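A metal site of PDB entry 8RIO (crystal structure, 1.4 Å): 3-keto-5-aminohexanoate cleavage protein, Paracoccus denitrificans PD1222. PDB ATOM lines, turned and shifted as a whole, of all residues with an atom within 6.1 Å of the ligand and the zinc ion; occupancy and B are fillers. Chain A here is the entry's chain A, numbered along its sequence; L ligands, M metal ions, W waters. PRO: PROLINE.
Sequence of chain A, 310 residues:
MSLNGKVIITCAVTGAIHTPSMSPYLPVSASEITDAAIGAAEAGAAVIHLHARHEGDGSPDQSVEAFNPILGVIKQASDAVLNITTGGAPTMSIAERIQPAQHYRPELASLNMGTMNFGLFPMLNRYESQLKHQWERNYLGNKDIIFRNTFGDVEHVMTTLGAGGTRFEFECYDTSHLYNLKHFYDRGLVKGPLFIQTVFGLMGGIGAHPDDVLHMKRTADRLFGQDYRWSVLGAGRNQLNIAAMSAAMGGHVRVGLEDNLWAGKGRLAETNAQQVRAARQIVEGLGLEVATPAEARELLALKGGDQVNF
OE2 of Glu 258 binds the zinc ion, at 2.0 Å.
NE2 of His 49 binds the zinc ion (2.1 Å).
NE2 of His 51 binds the zinc ion, at 2.1 Å.
The zinc ion is bound by O of the ligand (2.2 Å).
The zinc ion is bound by water W1 (2.3 Å).
The zinc ion has five donor atoms within binding distance.
Slightly farther from the zinc ion lies OXT of the ligand (2.7 Å).
Water W1 lies within hydrogen-bond range of the side-chain carboxylate (OE2) of Glu 171, the guanidinium group (NH2) of Arg 254 and an oxygen (OXT) of the ligand.
Water W4 lies within hydrogen-bond range of OXT of the ligand, OG of Ser 110 and OE1 of Glu 171.
The guanidinium group of Arg 254 sits close to the side-chain carboxylate of Glu 258 (3.3 Å).
The backbone NH (N) of Gly 15 lies close to the side-chain carboxylate (OE1) of Glu 258.
N of Glu 258 is in hydrogen-bond range of O of Ala 12.
A ring nitrogen (ND1) of His 49 is in hydrogen-bond range of the guanidinium group (NH1) of Arg 254, 3.3 Å away.
NE2 of His 51 sits close to OG1 of Thr 85 (3.4 Å).
The backbone NH (N) of Thr 85 lies within hydrogen-bond range of the backbone carbonyl oxygen (O) of Leu 50, at 3.1 Å.
The side-chain carboxylate (OE1) of Glu 171 sits at hydrogen-bond distance from the side-chain hydroxyl (OH) of Tyr 173 (2.7 Å).
The side-chain hydroxyl (OG1) of Thr 86 is in hydrogen-bond range of the backbone carbonyl oxygen (O) of Ser 110.
The side-chain hydroxyl (OG1) of Thr 85 sits at hydrogen-bond distance from an oxygen (OXT) of the ligand (2.8 Å).
Three residues have an atom within 4 Å of the zinc ion: His 49, His 51 and Glu 258.
Merely in contact with the ligand: Phe 147 (3.2 Å), Glu 171 (3.4 Å), Tyr 173 (3.5 Å), Ser 110 (3.5 Å), Asn 112 (3.8 Å) and Ile 17 (3.98 Å).
Of the 22 residues printed, 10 come within 4 Å of the ligand.
The nearest printed residue that does not touch the ligand is Gly 87 (4.1 Å).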
ATOM      1  N   ALA A  12      -6.212  -4.916   3.637  1.00  0.00           N
ATOM      2  CA  ALA A  12      -4.980  -4.764   2.839  1.00  0.00           C
ATOM      3  C   ALA A  12      -4.771  -3.265   2.608  1.00  0.00           C
ATOM      4  O   ALA A  12      -5.497  -2.648   1.821  1.00  0.00           O
ATOM      5  CB  ALA A  12      -5.079  -5.563   1.514  1.00  0.00           C
ATOM      6  N   GLY A  15      -0.689  -2.117  -0.605  1.00  0.00           N
ATOM      7  CA  GLY A  15      -0.436  -2.932  -1.823  1.00  0.00           C
ATOM      8  C   GLY A  15       0.662  -2.372  -2.718  1.00  0.00           C
ATOM      9  O   GLY A  15       1.516  -1.568  -2.297  1.00  0.00           O
ATOM     10  N   ALA A  16       0.604  -2.831  -3.975  1.00  0.00           N
ATOM     11  CA  ALA A  16       1.542  -2.457  -5.015  1.00  0.00           C
ATOM     12  C   ALA A  16       0.836  -2.253  -6.348  1.00  0.00           C
ATOM     13  O   ALA A  16       1.507  -1.892  -7.315  1.00  0.00           O
ATOM     14  CB  ALA A  16       2.649  -3.550  -5.152  1.00  0.00           C
ATOM     15  N   ILE A  17      -0.473  -2.457  -6.426  1.00  0.00           N
ATOM     16  CA  ILE A  17      -1.207  -2.302  -7.694  1.00  0.00           C
ATOM     17  C   ILE A  17      -1.655  -0.855  -7.911  1.00  0.00           C
ATOM     18  O   ILE A  17      -1.485  -0.312  -8.998  1.00  0.00           O
ATOM     19  CB  ILE A  17      -2.389  -3.284  -7.720  1.00  0.00           C
ATOM     20  CG1 ILE A  17      -1.821  -4.697  -8.074  1.00  0.00           C
ATOM     21  CG2 ILE A  17      -3.476  -2.804  -8.757  1.00  0.00           C
ATOM     22  CD1 ILE A  17      -2.846  -5.827  -7.875  1.00  0.00           C
ATOM     23  N   HIS A  49      -2.952  -7.079   5.909  1.00  0.00           N
ATOM     24  CA  HIS A  49      -2.061  -7.480   4.791  1.00  0.00           C
ATOM     25  C   HIS A  49      -1.210  -6.289   4.377  1.00  0.00           C
ATOM     26  O   HIS A  49      -1.746  -5.231   4.006  1.00  0.00           O
ATOM     27  CB  HIS A  49      -2.966  -7.986   3.655  1.00  0.00           C
ATOM     28  CG  HIS A  49      -2.277  -8.307   2.364  1.00  0.00           C
ATOM     29  ND1 HIS A  49      -2.282  -9.589   1.838  1.00  0.00           N
ATOM     30  CD2 HIS A  49      -1.809  -7.505   1.365  1.00  0.00           C
ATOM     31  CE1 HIS A  49      -1.687  -9.581   0.657  1.00  0.00           C
ATOM     32  NE2 HIS A  49      -1.390  -8.322   0.350  1.00  0.00           N
ATOM     33  N   LEU A  50       0.129  -6.432   4.472  1.00  0.00           N
ATOM     34  CA  LEU A  50       1.067  -5.333   4.426  1.00  0.00           C
ATOM     35  C   LEU A  50       2.013  -5.423   3.246  1.00  0.00           C
ATOM     36  O   LEU A  50       2.567  -6.492   2.955  1.00  0.00           O
ATOM     37  CB  LEU A  50       1.905  -5.391   5.710  1.00  0.00           C
ATOM     38  CG  LEU A  50       1.099  -4.944   6.950  1.00  0.00           C
ATOM     39  CD1 LEU A  50       1.911  -5.346   8.238  1.00  0.00           C
ATOM     40  CD2 LEU A  50       0.843  -3.456   6.955  1.00  0.00           C
ATOM     41  N   HIS A  51       2.229  -4.264   2.611  1.00  0.00           N
ATOM     42  CA  HIS A  51       3.345  -3.984   1.710  1.00  0.00           C
ATOM     43  C   HIS A  51       4.010  -2.716   2.205  1.00  0.00           C
ATOM     44  O   HIS A  51       3.444  -1.974   3.019  1.00  0.00           O
ATOM     45  CB  HIS A  51       2.842  -3.649   0.299  1.00  0.00           C
ATOM     46  CG  HIS A  51       2.141  -4.784  -0.415  1.00  0.00           C
ATOM     47  ND1 HIS A  51       2.534  -5.197  -1.675  1.00  0.00           N
ATOM     48  CD2 HIS A  51       1.054  -5.544  -0.099  1.00  0.00           C
ATOM     49  CE1 HIS A  51       1.710  -6.132  -2.114  1.00  0.00           C
ATOM     50  NE2 HIS A  51       0.827  -6.378  -1.161  1.00  0.00           N
ATOM     51  N   THR A  85       3.273  -9.522   2.466  1.00  0.00           N
ATOM     52  CA  THR A  85       3.261  -9.938   1.069  1.00  0.00           C
ATOM     53  C   THR A  85       4.526 -10.701   0.674  1.00  0.00           C
ATOM     54  O   THR A  85       5.624 -10.413   1.177  1.00  0.00           O
ATOM     55  CB  THR A  85       3.119  -8.695   0.169  1.00  0.00           C
ATOM     56  OG1 THR A  85       2.877  -9.116  -1.173  1.00  0.00           O
ATOM     57  CG2 THR A  85       4.349  -7.786   0.183  1.00  0.00           C
ATOM     58  N   THR A  86       4.367 -11.606  -0.300  1.00  0.00           N
ATOM     59  CA  THR A  86       5.465 -12.204  -1.056  1.00  0.00           C
ATOM     60  C   THR A  86       5.429 -11.847  -2.518  1.00  0.00           C
ATOM     61  O   THR A  86       6.092 -12.506  -3.323  1.00  0.00           O
ATOM     62  CB  THR A  86       5.548 -13.731  -0.872  1.00  0.00           C
ATOM     63  OG1 THR A  86       4.369 -14.342  -1.462  1.00  0.00           O
ATOM     64  CG2 THR A  86       5.697 -14.090   0.574  1.00  0.00           C
ATOM     65  N   GLY A  87       4.696 -10.778  -2.863  1.00  0.00           N
ATOM     66  CA  GLY A  87       4.693 -10.325  -4.247  1.00  0.00           C
ATOM     67  C   GLY A  87       5.933  -9.528  -4.542  1.00  0.00           C
ATOM     68  O   GLY A  87       6.677  -9.162  -3.653  1.00  0.00           O
ATOM     69  N   GLY A  88       6.086  -9.163  -5.785  1.00  0.00           N
ATOM     70  CA  GLY A  88       7.178  -8.253  -6.092  1.00  0.00           C
ATOM     71  C   GLY A  88       7.169  -7.964  -7.565  1.00  0.00           C
ATOM     72  O   GLY A  88       6.345  -8.487  -8.317  1.00  0.00           O
ATOM     73  N   ARG A  97      11.841 -12.113  -3.358  1.00  0.00           N
ATOM     74  CA  ARG A  97      10.496 -11.719  -2.947  1.00  0.00           C
ATOM     75  C   ARG A  97      10.144 -12.210  -1.545  1.00  0.00           C
ATOM     76  O   ARG A  97       9.374 -11.534  -0.833  1.00  0.00           O
ATOM     77  CB  ARG A  97       9.471 -12.328  -3.920  1.00  0.00           C
ATOM     78  CG  ARG A  97       9.380 -11.449  -5.195  1.00  0.00           C
ATOM     79  CD  ARG A  97       8.624 -12.238  -6.324  1.00  0.00           C
ATOM     80  NE  ARG A  97       7.320 -12.629  -5.827  1.00  0.00           N
ATOM     81  CZ  ARG A  97       6.512 -13.457  -6.466  1.00  0.00           C
ATOM     82  NH1 ARG A  97       6.809 -13.882  -7.699  1.00  0.00           N
ATOM     83  NH2 ARG A  97       5.391 -13.832  -5.874  1.00  0.00           N
ATOM     84  N   SER A 110       1.342 -13.741   2.297  1.00  0.00           N
ATOM     85  CA  SER A 110       0.481 -13.985   1.141  1.00  0.00           C
ATOM     86  C   SER A 110       1.193 -14.892   0.155  1.00  0.00           C
ATOM     87  O   SER A 110       2.418 -14.987   0.163  1.00  0.00           O
ATOM     88  CB  SER A 110       0.140 -12.631   0.494  1.00  0.00           C
ATOM     89  OG  SER A 110       1.261 -12.152  -0.232  1.00  0.00           O
ATOM     90  N   ASN A 112       0.600 -15.992  -3.946  1.00  0.00           N
ATOM     91  CA  ASN A 112      -0.149 -16.079  -5.181  1.00  0.00           C
ATOM     92  C   ASN A 112       0.068 -17.468  -5.789  1.00  0.00           C
ATOM     93  O   ASN A 112       1.201 -17.916  -5.962  1.00  0.00           O
ATOM     94  CB  ASN A 112       0.326 -14.981  -6.130  1.00  0.00           C
ATOM     95  CG  ASN A 112      -0.509 -14.890  -7.411  1.00  0.00           C
ATOM     96  OD1 ASN A 112      -1.217 -15.838  -7.812  1.00  0.00           O
ATOM     97  ND2 ASN A 112      -0.409 -13.760  -8.085  1.00  0.00           N
ATOM     98  N   PHE A 147       2.620 -11.692 -13.237  1.00  0.00           N
ATOM     99  CA  PHE A 147       2.956 -12.104 -11.868  1.00  0.00           C
ATOM    100  C   PHE A 147       3.435 -13.539 -12.009  1.00  0.00           C
ATOM    101  O   PHE A 147       2.648 -14.412 -12.393  1.00  0.00           O
ATOM    102  CB  PHE A 147       1.739 -12.062 -10.948  1.00  0.00           C
ATOM    103  CG  PHE A 147       1.041 -10.682 -10.816  1.00  0.00           C
ATOM    104  CD1 PHE A 147       1.754  -9.502 -10.990  1.00  0.00           C
ATOM    105  CD2 PHE A 147      -0.291 -10.604 -10.485  1.00  0.00           C
ATOM    106  CE1 PHE A 147       1.108  -8.231 -10.843  1.00  0.00           C
ATOM    107  CE2 PHE A 147      -0.953  -9.318 -10.349  1.00  0.00           C
ATOM    108  CZ  PHE A 147      -0.220  -8.173 -10.519  1.00  0.00           C
ATOM    109  N   ASN A 149       4.560 -17.097 -10.705  1.00  0.00           N
ATOM    110  CA  ASN A 149       4.500 -17.963  -9.535  1.00  0.00           C
ATOM    111  C   ASN A 149       4.406 -19.386 -10.059  1.00  0.00           C
ATOM    112  O   ASN A 149       3.337 -20.014 -10.062  1.00  0.00           O
ATOM    113  CB  ASN A 149       3.291 -17.651  -8.651  1.00  0.00           C
ATOM    114  CG  ASN A 149       3.317 -16.231  -8.158  1.00  0.00           C
ATOM    115  OD1 ASN A 149       4.101 -15.896  -7.268  1.00  0.00           O
ATOM    116  ND2 ASN A 149       2.562 -15.357  -8.809  1.00  0.00           N
ATOM    117  N   GLU A 171      -3.669 -16.732  -2.256  1.00  0.00           N
ATOM    118  CA  GLU A 171      -4.444 -15.883  -3.147  1.00  0.00           C
ATOM    119  C   GLU A 171      -4.697 -16.609  -4.465  1.00  0.00           C
ATOM    120  O   GLU A 171      -3.760 -16.950  -5.169  1.00  0.00           O
ATOM    121  CB  GLU A 171      -3.684 -14.573  -3.386  1.00  0.00           C
ATOM    122  CG  GLU A 171      -3.501 -13.696  -2.121  1.00  0.00           C
ATOM    123  CD  GLU A 171      -2.813 -12.409  -2.438  1.00  0.00           C
ATOM    124  OE1 GLU A 171      -2.116 -12.328  -3.484  1.00  0.00           O
ATOM    125  OE2 GLU A 171      -2.861 -11.533  -1.592  1.00  0.00           O
ATOM    126  N   TYR A 173      -6.697 -16.449  -7.975  1.00  0.00           N
ATOM    127  CA  TYR A 173      -7.274 -15.439  -8.877  1.00  0.00           C
ATOM    128  C   TYR A 173      -8.115 -16.064  -9.956  1.00  0.00           C
ATOM    129  O   TYR A 173      -8.686 -15.333 -10.769  1.00  0.00           O
ATOM    130  CB  TYR A 173      -6.123 -14.597  -9.508  1.00  0.00           C
ATOM    131  CG  TYR A 173      -5.328 -13.762  -8.549  1.00  0.00           C
ATOM    132  CD1 TYR A 173      -4.353 -14.315  -7.749  1.00  0.00           C
ATOM    133  CD2 TYR A 173      -5.588 -12.414  -8.423  1.00  0.00           C
ATOM    134  CE1 TYR A 173      -3.648 -13.551  -6.804  1.00  0.00           C
ATOM    135  CE2 TYR A 173      -4.862 -11.627  -7.505  1.00  0.00           C
ATOM    136  CZ  TYR A 173      -3.912 -12.222  -6.724  1.00  0.00           C
ATOM    137  OH  TYR A 173      -3.211 -11.454  -5.747  1.00  0.00           O
ATOM    138  N   LEU A 202      -9.905  -8.590 -11.157  1.00  0.00           N
ATOM    139  CA  LEU A 202      -8.705  -7.981 -11.685  1.00  0.00           C
ATOM    140  C   LEU A 202      -8.538  -8.366 -13.146  1.00  0.00           C
ATOM    141  O   LEU A 202      -8.894  -9.468 -13.565  1.00  0.00           O
ATOM    142  CB  LEU A 202      -7.462  -8.449 -10.910  1.00  0.00           C
ATOM    143  CG  LEU A 202      -7.410  -7.921  -9.481  1.00  0.00           C
ATOM    144  CD1 LEU A 202      -6.095  -8.418  -8.752  1.00  0.00           C
ATOM    145  CD2 LEU A 202      -7.362  -6.428  -9.470  1.00  0.00           C
ATOM    146  N   ARG A 254     -12.218  -9.604   2.782  1.00  0.00           N
ATOM    147  CA  ARG A 254     -11.055  -8.735   2.670  1.00  0.00           C
ATOM    148  C   ARG A 254     -11.496  -7.401   2.083  1.00  0.00           C
ATOM    149  O   ARG A 254     -12.163  -7.369   1.037  1.00  0.00           O
ATOM    150  CB  ARG A 254      -9.962  -9.393   1.813  1.00  0.00           C
ATOM    151  CG  ARG A 254      -8.751  -8.505   1.545  1.00  0.00           C
ATOM    152  CD  ARG A 254      -7.623  -9.342   0.949  1.00  0.00           C
ATOM    153  NE  ARG A 254      -6.709  -8.373   0.294  1.00  0.00           N
ATOM    154  CZ  ARG A 254      -5.540  -8.742  -0.231  1.00  0.00           C
ATOM    155  NH1 ARG A 254      -5.053  -9.965  -0.004  1.00  0.00           N
ATOM    156  NH2 ARG A 254      -4.897  -7.881  -1.061  1.00  0.00           N
ATOM    157  N   GLU A 258      -5.526  -1.179  -0.763  1.00  0.00           N
ATOM    158  CA  GLU A 258      -4.727  -1.961  -1.726  1.00  0.00           C
ATOM    159  C   GLU A 258      -5.620  -2.463  -2.854  1.00  0.00           C
ATOM    160  O   GLU A 258      -5.189  -2.571  -3.997  1.00  0.00           O
ATOM    161  CB  GLU A 258      -4.112  -3.169  -0.994  1.00  0.00           C
ATOM    162  CG  GLU A 258      -3.618  -4.242  -1.966  1.00  0.00           C
ATOM    163  CD  GLU A 258      -2.628  -5.201  -1.351  1.00  0.00           C
ATOM    164  OE1 GLU A 258      -2.198  -5.013  -0.215  1.00  0.00           O
ATOM    165  OE2 GLU A 258      -2.266  -6.204  -2.050  1.00  0.00           O
ATOM    166  N   ASP A 259      -6.881  -2.772  -2.504  1.00  0.00           N
ATOM    167  CA  ASP A 259      -7.786  -3.518  -3.372  1.00  0.00           C
ATOM    168  C   ASP A 259      -8.849  -2.642  -4.042  1.00  0.00           C
ATOM    169  O   ASP A 259      -9.300  -2.969  -5.146  1.00  0.00           O
ATOM    170  CB  ASP A 259      -8.542  -4.576  -2.516  1.00  0.00           C
ATOM    171  CG  ASP A 259      -7.624  -5.566  -1.832  1.00  0.00           C
ATOM    172  OD1 ASP A 259      -6.538  -5.850  -2.394  1.00  0.00           O
ATOM    173  OD2 ASP A 259      -8.025  -6.124  -0.812  1.00  0.00           O
HETATM  174  N   PRO L   1      -0.947  -8.750  -5.763  1.00  0.00           N
HETATM  175  CA  PRO L   1      -0.324  -9.724  -4.845  1.00  0.00           C
HETATM  176  C   PRO L   1       0.025  -8.998  -3.572  1.00  0.00           C
HETATM  177  O   PRO L   1      -0.293  -7.772  -3.637  1.00  0.00           O
HETATM  178  CB  PRO L   1       0.874 -10.215  -5.648  1.00  0.00           C
HETATM  179  CG  PRO L   1       0.343 -10.227  -7.065  1.00  0.00           C
HETATM  180  CD  PRO L   1      -0.676  -9.085  -7.166  1.00  0.00           C
HETATM  181  OXT PRO L   1       0.482  -9.585  -2.514  1.00  0.00           O
HETATM  182 ZN    ZN M   1      -0.907  -7.555  -1.520  1.00  0.00          ZN
HETATM  183  O   HOH W   1      -2.561  -9.016  -2.266  1.00  0.00           O
HETATM  184  O   HOH W   2       2.476 -12.749  -7.444  1.00  0.00           O
HETATM  185  O   HOH W   3      -1.087  -5.035  -4.498  1.00  0.00           O
HETATM  186  O   HOH W   4       0.631 -12.081  -2.942  1.00  0.00           O
HETATM  187  O   HOH W   5       0.706  -6.413  -5.893  1.00  0.00           O
